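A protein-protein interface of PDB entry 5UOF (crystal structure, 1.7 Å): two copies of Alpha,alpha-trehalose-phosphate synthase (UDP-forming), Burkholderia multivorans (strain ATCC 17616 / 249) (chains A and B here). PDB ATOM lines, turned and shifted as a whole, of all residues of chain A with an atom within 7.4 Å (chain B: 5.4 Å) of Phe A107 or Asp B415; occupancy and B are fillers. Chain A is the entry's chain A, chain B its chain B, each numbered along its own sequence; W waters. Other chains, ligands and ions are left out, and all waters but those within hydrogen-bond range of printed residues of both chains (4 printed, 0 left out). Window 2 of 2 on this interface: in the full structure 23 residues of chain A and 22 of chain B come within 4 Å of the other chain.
No position is printed for both chains. Of the 9 pairs that touch across the chains among the printed residues, none has its exchanged pair printed and touching as well.
Of chain B, only Tyr B414 and Asp B415 come within 4 Å of Phe A107. Asp B415 touches just these residues of chain A: Phe A107 (3.5 Å), Arg A109 (3.1 Å) and Pro A177 (3.9 Å). Printed residues of chain A within 4 Å of Gln B418: Arg A109. Of the printed residues of chain B, Arg A109 touches Asp B415, Ser B417 and Gln B418. Printed residues of chain B within 4 Å of Leu A175: Tyr B414. Val A176 touches none of the printed residues of chain B. The nearest printed residue of chain B that does not touch Phe A107 is Leu B416 (5.7 Å).
Water W1 bridges the backbone carbonyl oxygen (O) of Pro A177 (2.7 Å) and the side-chain amide nitrogen (NE2) of Gln B418 (3.0 Å). Water W3 bridges O of Tyr B414 and N of Phe A107. Water W4 bridges the backbone NH (N) of Arg A109 (2.9 Å) and the side-chain hydroxyl (OG) of Ser B417 (3.5 Å). Water W2 lies within hydrogen-bond range of the backbone NH of Leu B416 (3.0 Å), the backbone carbonyl oxygen of Phe A107 (3.0 Å) and the backbone carbonyl oxygen of Tyr B414 (3.4 Å).
NH2 of Arg A109 lies close to N of Gln B418, at 3.2 Å. The side-chain carboxylate of Asp B415 lies within salt-bridge range of the guanidinium group of Arg A109 (3.1 Å).
O of Tyr B414 touches CB of Phe A107 (3.5 Å). Phe A107 touches Asp B415. C of Ser B417 touches NH2 of Arg A109, at 3.4 Å. Leu A175 touches Tyr B414. Pro A177 touches Asn B412 (CA to ND2, 3.8 Å). O of Tyr B414 touches CG of Pro A177 (3.9 Å). Pro A177 touches Asp B415 (CG to CB, 3.9 Å).
OD1 of Asn B412 sits at hydrogen-bond distance from N of Tyr B414, at 2.9 Å. The side-chain hydroxyl (OG) of Ser B417 is in hydrogen-bond range of the guanidinium group (NH1) of Arg B289 (3.0 Å). The backbone NH of Ser B417 sits at hydrogen-bond distance from the side-chain carboxylate of Asp B415 (3.0 Å). OD1 of Asp B415 is in hydrogen-bond range of N of Gln B418 (3.5 Å). The side-chain amide oxygen (OE1) of Gln B418 sits at hydrogen-bond distance from the backbone NH (N) of Asn B412 (3.0 Å).
Of the 17 printed residues of chain A, 4 touch a printed residue of chain B. Along chain A the printed residues that touch a printed residue of chain B span positions 107 to 177. Of the 9 printed residues of chain B, 5 touch a printed residue of chain A. Among the printed residues, 9 pairs touch across the chains. Among the printed residues, Asp or Glu carboxylates within 4 Å of a Lys or Arg side-chain nitrogen of the other chain: Arg A109 with Asp B415 (3.1 Å).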
ATOM      1  N   PHE A  89     -34.463  -7.050  24.948  1.00  0.00           N
ATOM      2  CA  PHE A  89     -34.189  -5.630  24.740  1.00  0.00           C
ATOM      3  C   PHE A  89     -34.649  -4.769  25.915  1.00  0.00           C
ATOM      4  O   PHE A  89     -33.947  -3.830  26.312  1.00  0.00           O
ATOM      5  CB  PHE A  89     -34.864  -5.173  23.440  1.00  0.00           C
ATOM      6  CG  PHE A  89     -34.864  -3.681  23.243  1.00  0.00           C
ATOM      7  CD1 PHE A  89     -33.738  -3.032  22.738  1.00  0.00           C
ATOM      8  CD2 PHE A  89     -35.987  -2.930  23.552  1.00  0.00           C
ATOM      9  CE1 PHE A  89     -33.739  -1.660  22.560  1.00  0.00           C
ATOM     10  CE2 PHE A  89     -36.005  -1.556  23.365  1.00  0.00           C
ATOM     11  CZ  PHE A  89     -34.870  -0.911  22.877  1.00  0.00           C
ATOM     12  N   ALA A  92     -32.148  -5.580  28.808  1.00  0.00           N
ATOM     13  CA  ALA A  92     -30.747  -5.422  28.437  1.00  0.00           C
ATOM     14  C   ALA A  92     -30.415  -4.027  27.939  1.00  0.00           C
ATOM     15  O   ALA A  92     -29.249  -3.635  28.001  1.00  0.00           O
ATOM     16  CB  ALA A  92     -30.348  -6.442  27.357  1.00  0.00           C
ATOM     17  N   THR A  93     -31.399  -3.276  27.437  1.00  0.00           N
ATOM     18  CA  THR A  93     -31.132  -1.965  26.851  1.00  0.00           C
ATOM     19  C   THR A  93     -31.969  -0.870  27.494  1.00  0.00           C
ATOM     20  O   THR A  93     -31.413   0.103  28.002  1.00  0.00           O
ATOM     21  CB  THR A  93     -31.387  -1.979  25.328  1.00  0.00           C
ATOM     22  OG1 THR A  93     -30.637  -3.026  24.714  1.00  0.00           O
ATOM     23  CG2 THR A  93     -30.969  -0.654  24.701  1.00  0.00           C
ATOM     24  N   LEU A 104     -24.070  -0.168  31.142  1.00  0.00           N
ATOM     25  CA  LEU A 104     -24.545  -1.539  31.285  1.00  0.00           C
ATOM     26  C   LEU A 104     -25.405  -1.990  30.116  1.00  0.00           C
ATOM     27  O   LEU A 104     -25.714  -3.187  30.011  1.00  0.00           O
ATOM     28  CB  LEU A 104     -25.347  -1.686  32.582  1.00  0.00           C
ATOM     29  CG  LEU A 104     -24.553  -1.437  33.863  1.00  0.00           C
ATOM     30  CD1 LEU A 104     -25.467  -1.620  35.073  1.00  0.00           C
ATOM     31  CD2 LEU A 104     -23.337  -2.343  33.950  1.00  0.00           C
ATOM     32  N   ALA A 105     -25.788  -1.067  29.241  1.00  0.00           N
ATOM     33  CA  ALA A 105     -26.687  -1.390  28.145  1.00  0.00           C
ATOM     34  C   ALA A 105     -25.978  -2.233  27.097  1.00  0.00           C
ATOM     35  O   ALA A 105     -24.788  -2.041  26.816  1.00  0.00           O
ATOM     36  CB  ALA A 105     -27.219  -0.109  27.507  1.00  0.00           C
ATOM     37  N   ARG A 106     -26.722  -3.179  26.521  1.00  0.00           N
ATOM     38  CA  ARG A 106     -26.225  -4.075  25.472  1.00  0.00           C
ATOM     39  C   ARG A 106     -27.294  -4.146  24.385  1.00  0.00           C
ATOM     40  O   ARG A 106     -28.145  -5.041  24.396  1.00  0.00           O
ATOM     41  CB  ARG A 106     -25.901  -5.464  26.022  1.00  0.00           C
ATOM     42  CG  ARG A 106     -24.895  -5.474  27.179  1.00  0.00           C
ATOM     43  CD  ARG A 106     -23.499  -5.032  26.731  1.00  0.00           C
ATOM     44  NE  ARG A 106     -22.510  -5.178  27.805  1.00  0.00           N
ATOM     45  CZ  ARG A 106     -22.098  -4.194  28.604  1.00  0.00           C
ATOM     46  NH1 ARG A 106     -22.571  -2.961  28.463  1.00  0.00           N
ATOM     47  NH2 ARG A 106     -21.198  -4.442  29.548  1.00  0.00           N
ATOM     48  N   PHE A 107     -27.226  -3.241  23.412  1.00  0.00           N
ATOM     49  CA  PHE A 107     -28.204  -3.250  22.332  1.00  0.00           C
ATOM     50  C   PHE A 107     -27.944  -4.363  21.315  1.00  0.00           C
ATOM     51  O   PHE A 107     -26.811  -4.592  20.884  1.00  0.00           O
ATOM     52  CB  PHE A 107     -28.227  -1.906  21.610  1.00  0.00           C
ATOM     53  CG  PHE A 107     -29.146  -1.913  20.421  1.00  0.00           C
ATOM     54  CD1 PHE A 107     -30.524  -1.845  20.599  1.00  0.00           C
ATOM     55  CD2 PHE A 107     -28.641  -2.009  19.137  1.00  0.00           C
ATOM     56  CE1 PHE A 107     -31.394  -1.874  19.500  1.00  0.00           C
ATOM     57  CE2 PHE A 107     -29.493  -2.041  18.040  1.00  0.00           C
ATOM     58  CZ  PHE A 107     -30.875  -1.963  18.222  1.00  0.00           C
ATOM     59  N   ASP A 108     -29.013  -5.035  20.902  1.00  0.00           N
ATOM     60  CA  ASP A 108     -28.916  -6.084  19.893  1.00  0.00           C
ATOM     61  C   ASP A 108     -30.112  -5.982  18.958  1.00  0.00           C
ATOM     62  O   ASP A 108     -31.258  -5.995  19.412  1.00  0.00           O
ATOM     63  CB  ASP A 108     -28.853  -7.472  20.538  1.00  0.00           C
ATOM     64  CG  ASP A 108     -28.843  -8.588  19.511  1.00  0.00           C
ATOM     65  OD1 ASP A 108     -27.768  -8.912  18.959  1.00  0.00           O
ATOM     66  OD2 ASP A 108     -29.919  -9.124  19.238  1.00  0.00           O
ATOM     67  N   ARG A 109     -29.845  -5.892  17.653  1.00  0.00           N
ATOM     68  CA  ARG A 109     -30.931  -5.683  16.696  1.00  0.00           C
ATOM     69  C   ARG A 109     -31.977  -6.782  16.783  1.00  0.00           C
ATOM     70  O   ARG A 109     -33.179  -6.507  16.707  1.00  0.00           O
ATOM     71  CB  ARG A 109     -30.384  -5.598  15.270  1.00  0.00           C
ATOM     72  CG  ARG A 109     -29.723  -4.264  14.961  1.00  0.00           C
ATOM     73  CD  ARG A 109     -29.246  -4.183  13.491  1.00  0.00           C
ATOM     74  NE  ARG A 109     -28.543  -2.917  13.302  1.00  0.00           N
ATOM     75  CZ  ARG A 109     -27.966  -2.537  12.172  1.00  0.00           C
ATOM     76  NH1 ARG A 109     -27.991  -3.337  11.121  1.00  0.00           N
ATOM     77  NH2 ARG A 109     -27.346  -1.362  12.113  1.00  0.00           N
ATOM     78  N   GLN A 110     -31.546  -8.040  16.907  1.00  0.00           N
ATOM     79  CA  GLN A 110     -32.532  -9.114  16.889  1.00  0.00           C
ATOM     80  C   GLN A 110     -33.378  -9.097  18.152  1.00  0.00           C
ATOM     81  O   GLN A 110     -34.578  -9.394  18.095  1.00  0.00           O
ATOM     82  CB  GLN A 110     -31.852 -10.472  16.705  1.00  0.00           C
ATOM     83  CG  GLN A 110     -31.028 -10.589  15.433  1.00  0.00           C
ATOM     84  CD  GLN A 110     -31.707  -9.965  14.226  1.00  0.00           C
ATOM     85  OE1 GLN A 110     -32.868 -10.256  13.927  1.00  0.00           O
ATOM     86  NE2 GLN A 110     -30.979  -9.097  13.523  1.00  0.00           N
ATOM     87  N   GLU A 111     -32.783  -8.738  19.292  1.00  0.00           N
ATOM     88  CA  GLU A 111     -33.575  -8.590  20.512  1.00  0.00           C
ATOM     89  C   GLU A 111     -34.598  -7.473  20.370  1.00  0.00           C
ATOM     90  O   GLU A 111     -35.744  -7.610  20.809  1.00  0.00           O
ATOM     91  CB  GLU A 111     -32.666  -8.328  21.718  1.00  0.00           C
ATOM     92  CG  GLU A 111     -31.841  -9.533  22.121  1.00  0.00           C
ATOM     93  CD  GLU A 111     -31.018  -9.287  23.374  1.00  0.00           C
ATOM     94  OE1 GLU A 111     -30.513 -10.269  23.959  1.00  0.00           O
ATOM     95  OE2 GLU A 111     -30.894  -8.119  23.779  1.00  0.00           O
ATOM     96  N   TYR A 112     -34.206  -6.360  19.744  1.00  0.00           N
ATOM     97  CA  TYR A 112     -35.150  -5.269  19.540  1.00  0.00           C
ATOM     98  C   TYR A 112     -36.295  -5.702  18.633  1.00  0.00           C
ATOM     99  O   TYR A 112     -37.463  -5.405  18.917  1.00  0.00           O
ATOM    100  CB  TYR A 112     -34.425  -4.039  18.972  1.00  0.00           C
ATOM    101  CG  TYR A 112     -35.351  -2.864  18.748  1.00  0.00           C
ATOM    102  CD1 TYR A 112     -36.131  -2.362  19.792  1.00  0.00           C
ATOM    103  CD2 TYR A 112     -35.455  -2.260  17.504  1.00  0.00           C
ATOM    104  CE1 TYR A 112     -36.993  -1.301  19.590  1.00  0.00           C
ATOM    105  CE2 TYR A 112     -36.321  -1.188  17.293  1.00  0.00           C
ATOM    106  CZ  TYR A 112     -37.083  -0.719  18.342  1.00  0.00           C
ATOM    107  OH  TYR A 112     -37.926   0.343  18.138  1.00  0.00           O
ATOM    108  N   ALA A 113     -35.983  -6.410  17.541  1.00  0.00           N
ATOM    109  CA  ALA A 113     -37.046  -6.953  16.699  1.00  0.00           C
ATOM    110  C   ALA A 113     -37.965  -7.863  17.504  1.00  0.00           C
ATOM    111  O   ALA A 113     -39.187  -7.861  17.302  1.00  0.00           O
ATOM    112  CB  ALA A 113     -36.460  -7.714  15.509  1.00  0.00           C
ATOM    113  N   LEU A 175     -28.658   6.960  23.953  1.00  0.00           N
ATOM    114  CA  LEU A 175     -27.864   5.747  24.087  1.00  0.00           C
ATOM    115  C   LEU A 175     -28.640   4.508  23.659  1.00  0.00           C
ATOM    116  O   LEU A 175     -28.026   3.474  23.386  1.00  0.00           O
ATOM    117  CB  LEU A 175     -27.381   5.595  25.525  1.00  0.00           C
ATOM    118  CG  LEU A 175     -26.530   6.794  25.967  1.00  0.00           C
ATOM    119  CD1 LEU A 175     -26.104   6.651  27.419  1.00  0.00           C
ATOM    120  CD2 LEU A 175     -25.342   6.961  25.069  1.00  0.00           C
ATOM    121  N   VAL A 176     -29.966   4.585  23.621  1.00  0.00           N
ATOM    122  CA  VAL A 176     -30.798   3.528  23.040  1.00  0.00           C
ATOM    123  C   VAL A 176     -30.849   3.760  21.534  1.00  0.00           C
ATOM    124  O   VAL A 176     -31.448   4.748  21.100  1.00  0.00           O
ATOM    125  CB  VAL A 176     -32.220   3.543  23.630  1.00  0.00           C
ATOM    126  CG1 VAL A 176     -33.065   2.452  22.984  1.00  0.00           C
ATOM    127  CG2 VAL A 176     -32.204   3.375  25.147  1.00  0.00           C
ATOM    128  N   PRO A 177     -30.256   2.911  20.698  1.00  0.00           N
ATOM    129  CA  PRO A 177     -30.153   3.248  19.262  1.00  0.00           C
ATOM    130  C   PRO A 177     -31.508   3.523  18.618  1.00  0.00           C
ATOM    131  O   PRO A 177     -31.621   4.475  17.831  1.00  0.00           O
ATOM    132  CB  PRO A 177     -29.448   2.019  18.660  1.00  0.00           C
ATOM    133  CG  PRO A 177     -28.540   1.554  19.807  1.00  0.00           C
ATOM    134  CD  PRO A 177     -29.408   1.758  21.058  1.00  0.00           C
ATOM    135  N   PRO A 178     -32.592   2.758  18.928  1.00  0.00           N
ATOM    136  CA  PRO A 178     -33.892   3.103  18.313  1.00  0.00           C
ATOM    137  C   PRO A 178     -34.716   4.147  19.077  1.00  0.00           C
ATOM    138  O   PRO A 178     -35.953   4.112  19.053  1.00  0.00           O
ATOM    139  CB  PRO A 178     -34.617   1.751  18.264  1.00  0.00           C
ATOM    140  CG  PRO A 178     -34.112   1.037  19.487  1.00  0.00           C
ATOM    141  CD  PRO A 178     -32.645   1.427  19.575  1.00  0.00           C
ATOM    142  N   ARG B 289     -16.802  -7.387  12.843  1.00  0.00           N
ATOM    143  CA  ARG B 289     -18.143  -7.742  12.399  1.00  0.00           C
ATOM    144  C   ARG B 289     -18.324  -7.425  10.922  1.00  0.00           C
ATOM    145  O   ARG B 289     -18.951  -8.196  10.192  1.00  0.00           O
ATOM    146  CB  ARG B 289     -19.199  -7.022  13.238  1.00  0.00           C
ATOM    147  CG  ARG B 289     -20.645  -7.371  12.840  1.00  0.00           C
ATOM    148  CD  ARG B 289     -21.620  -6.868  13.897  1.00  0.00           C
ATOM    149  NE  ARG B 289     -21.429  -7.551  15.175  1.00  0.00           N
ATOM    150  CZ  ARG B 289     -22.148  -7.306  16.267  1.00  0.00           C
ATOM    151  NH1 ARG B 289     -23.104  -6.388  16.245  1.00  0.00           N
ATOM    152  NH2 ARG B 289     -21.910  -7.977  17.387  1.00  0.00           N
ATOM    153  N   ASN B 412     -24.380   5.696  15.774  1.00  0.00           N
ATOM    154  CA  ASN B 412     -24.500   5.538  17.206  1.00  0.00           C
ATOM    155  C   ASN B 412     -23.597   4.375  17.579  1.00  0.00           C
ATOM    156  O   ASN B 412     -23.896   3.227  17.213  1.00  0.00           O
ATOM    157  CB  ASN B 412     -25.946   5.252  17.590  1.00  0.00           C
ATOM    158  CG  ASN B 412     -26.157   5.232  19.082  1.00  0.00           C
ATOM    159  OD1 ASN B 412     -25.295   4.781  19.833  1.00  0.00           O
ATOM    160  ND2 ASN B 412     -27.319   5.716  19.524  1.00  0.00           N
ATOM    161  N   PRO B 413     -22.484   4.612  18.271  1.00  0.00           N
ATOM    162  CA  PRO B 413     -21.550   3.513  18.551  1.00  0.00           C
ATOM    163  C   PRO B 413     -22.102   2.476  19.513  1.00  0.00           C
ATOM    164  O   PRO B 413     -21.467   1.428  19.687  1.00  0.00           O
ATOM    165  CB  PRO B 413     -20.328   4.232  19.139  1.00  0.00           C
ATOM    166  CG  PRO B 413     -20.861   5.544  19.654  1.00  0.00           C
ATOM    167  CD  PRO B 413     -21.975   5.920  18.724  1.00  0.00           C
ATOM    168  N   TYR B 414     -23.257   2.717  20.130  1.00  0.00           N
ATOM    169  CA  TYR B 414     -23.867   1.691  20.961  1.00  0.00           C
ATOM    170  C   TYR B 414     -24.632   0.657  20.145  1.00  0.00           C
ATOM    171  O   TYR B 414     -25.217  -0.264  20.724  1.00  0.00           O
ATOM    172  CB  TYR B 414     -24.761   2.346  22.018  1.00  0.00           C
ATOM    173  CG  TYR B 414     -23.926   3.135  23.011  1.00  0.00           C
ATOM    174  CD1 TYR B 414     -23.562   4.453  22.748  1.00  0.00           C
ATOM    175  CD2 TYR B 414     -23.463   2.544  24.180  1.00  0.00           C
ATOM    176  CE1 TYR B 414     -22.779   5.169  23.644  1.00  0.00           C
ATOM    177  CE2 TYR B 414     -22.688   3.254  25.081  1.00  0.00           C
ATOM    178  CZ  TYR B 414     -22.351   4.562  24.803  1.00  0.00           C
ATOM    179  OH  TYR B 414     -21.582   5.267  25.701  1.00  0.00           O
ATOM    180  N   ASP B 415     -24.629   0.780  18.820  1.00  0.00           N
ATOM    181  CA  ASP B 415     -25.071  -0.287  17.927  1.00  0.00           C
ATOM    182  C   ASP B 415     -23.837  -0.691  17.118  1.00  0.00           C
ATOM    183  O   ASP B 415     -23.483  -0.021  16.143  1.00  0.00           O
ATOM    184  CB  ASP B 415     -26.222   0.160  17.021  1.00  0.00           C
ATOM    185  CG  ASP B 415     -26.705  -0.949  16.121  1.00  0.00           C
ATOM    186  OD1 ASP B 415     -26.155  -2.057  16.237  1.00  0.00           O
ATOM    187  OD2 ASP B 415     -27.651  -0.744  15.320  1.00  0.00           O
ATOM    188  N   LEU B 416     -23.177  -1.781  17.533  1.00  0.00           N
ATOM    189  CA  LEU B 416     -22.015  -2.263  16.791  1.00  0.00           C
ATOM    190  C   LEU B 416     -22.352  -2.539  15.329  1.00  0.00           C
ATOM    191  O   LEU B 416     -21.510  -2.334  14.441  1.00  0.00           O
ATOM    192  CB  LEU B 416     -21.459  -3.528  17.444  1.00  0.00           C
ATOM    193  CG  LEU B 416     -19.983  -3.546  17.828  1.00  0.00           C
ATOM    194  CD1 LEU B 416     -19.701  -2.439  18.822  1.00  0.00           C
ATOM    195  CD2 LEU B 416     -19.620  -4.898  18.418  1.00  0.00           C
ATOM    196  N   SER B 417     -23.569  -3.012  15.049  1.00  0.00           N
ATOM    197  CA  SER B 417     -23.913  -3.299  13.657  1.00  0.00           C
ATOM    198  C   SER B 417     -24.055  -2.023  12.832  1.00  0.00           C
ATOM    199  O   SER B 417     -23.805  -2.049  11.624  1.00  0.00           O
ATOM    200  CB  SER B 417     -25.191  -4.136  13.574  1.00  0.00           C
ATOM    201  OG  SER B 417     -24.958  -5.442  14.046  1.00  0.00           O
ATOM    202  N   GLN B 418     -24.460  -0.907  13.452  1.00  0.00           N
ATOM    203  CA  GLN B 418     -24.461   0.374  12.744  1.00  0.00           C
ATOM    204  C   GLN B 418     -23.058   0.744  12.289  1.00  0.00           C
ATOM    205  O   GLN B 418     -22.868   1.272  11.185  1.00  0.00           O
ATOM    206  CB  GLN B 418     -24.997   1.495  13.630  1.00  0.00           C
ATOM    207  CG  GLN B 418     -26.480   1.744  13.579  1.00  0.00           C
ATOM    208  CD  GLN B 418     -26.852   3.074  14.230  1.00  0.00           C
ATOM    209  OE1 GLN B 418     -26.215   4.093  13.958  1.00  0.00           O
ATOM    210  NE2 GLN B 418     -27.886   3.070  15.082  1.00  0.00           N
ATOM    211  N   MET B 419     -22.066   0.520  13.144  1.00  0.00           N
ATOM    212  CA  MET B 419     -20.706   0.883  12.769  1.00  0.00           C
ATOM    213  C   MET B 419     -20.167  -0.057  11.701  1.00  0.00           C
ATOM    214  O   MET B 419     -19.516   0.386  10.752  1.00  0.00           O
ATOM    215  CB  MET B 419     -19.827   0.884  14.008  1.00  0.00           C
ATOM    216  CG  MET B 419     -20.321   1.917  14.988  1.00  0.00           C
ATOM    217  SD  MET B 419     -18.925   2.498  15.947  1.00  0.00           S
ATOM    218  CE  MET B 419     -18.782   1.140  17.058  1.00  0.00           C
HETATM  219  O   HOH W   1     -29.780   5.247  16.010  1.00  0.00           O
HETATM  220  O   HOH W   2     -24.342  -3.391  19.743  1.00  0.00           O
HETATM  221  O   HOH W   3     -25.374  -1.041  23.469  1.00  0.00           O
HETATM  222  O   HOH W   4     -27.116  -5.927  16.727  1.00  0.00           O
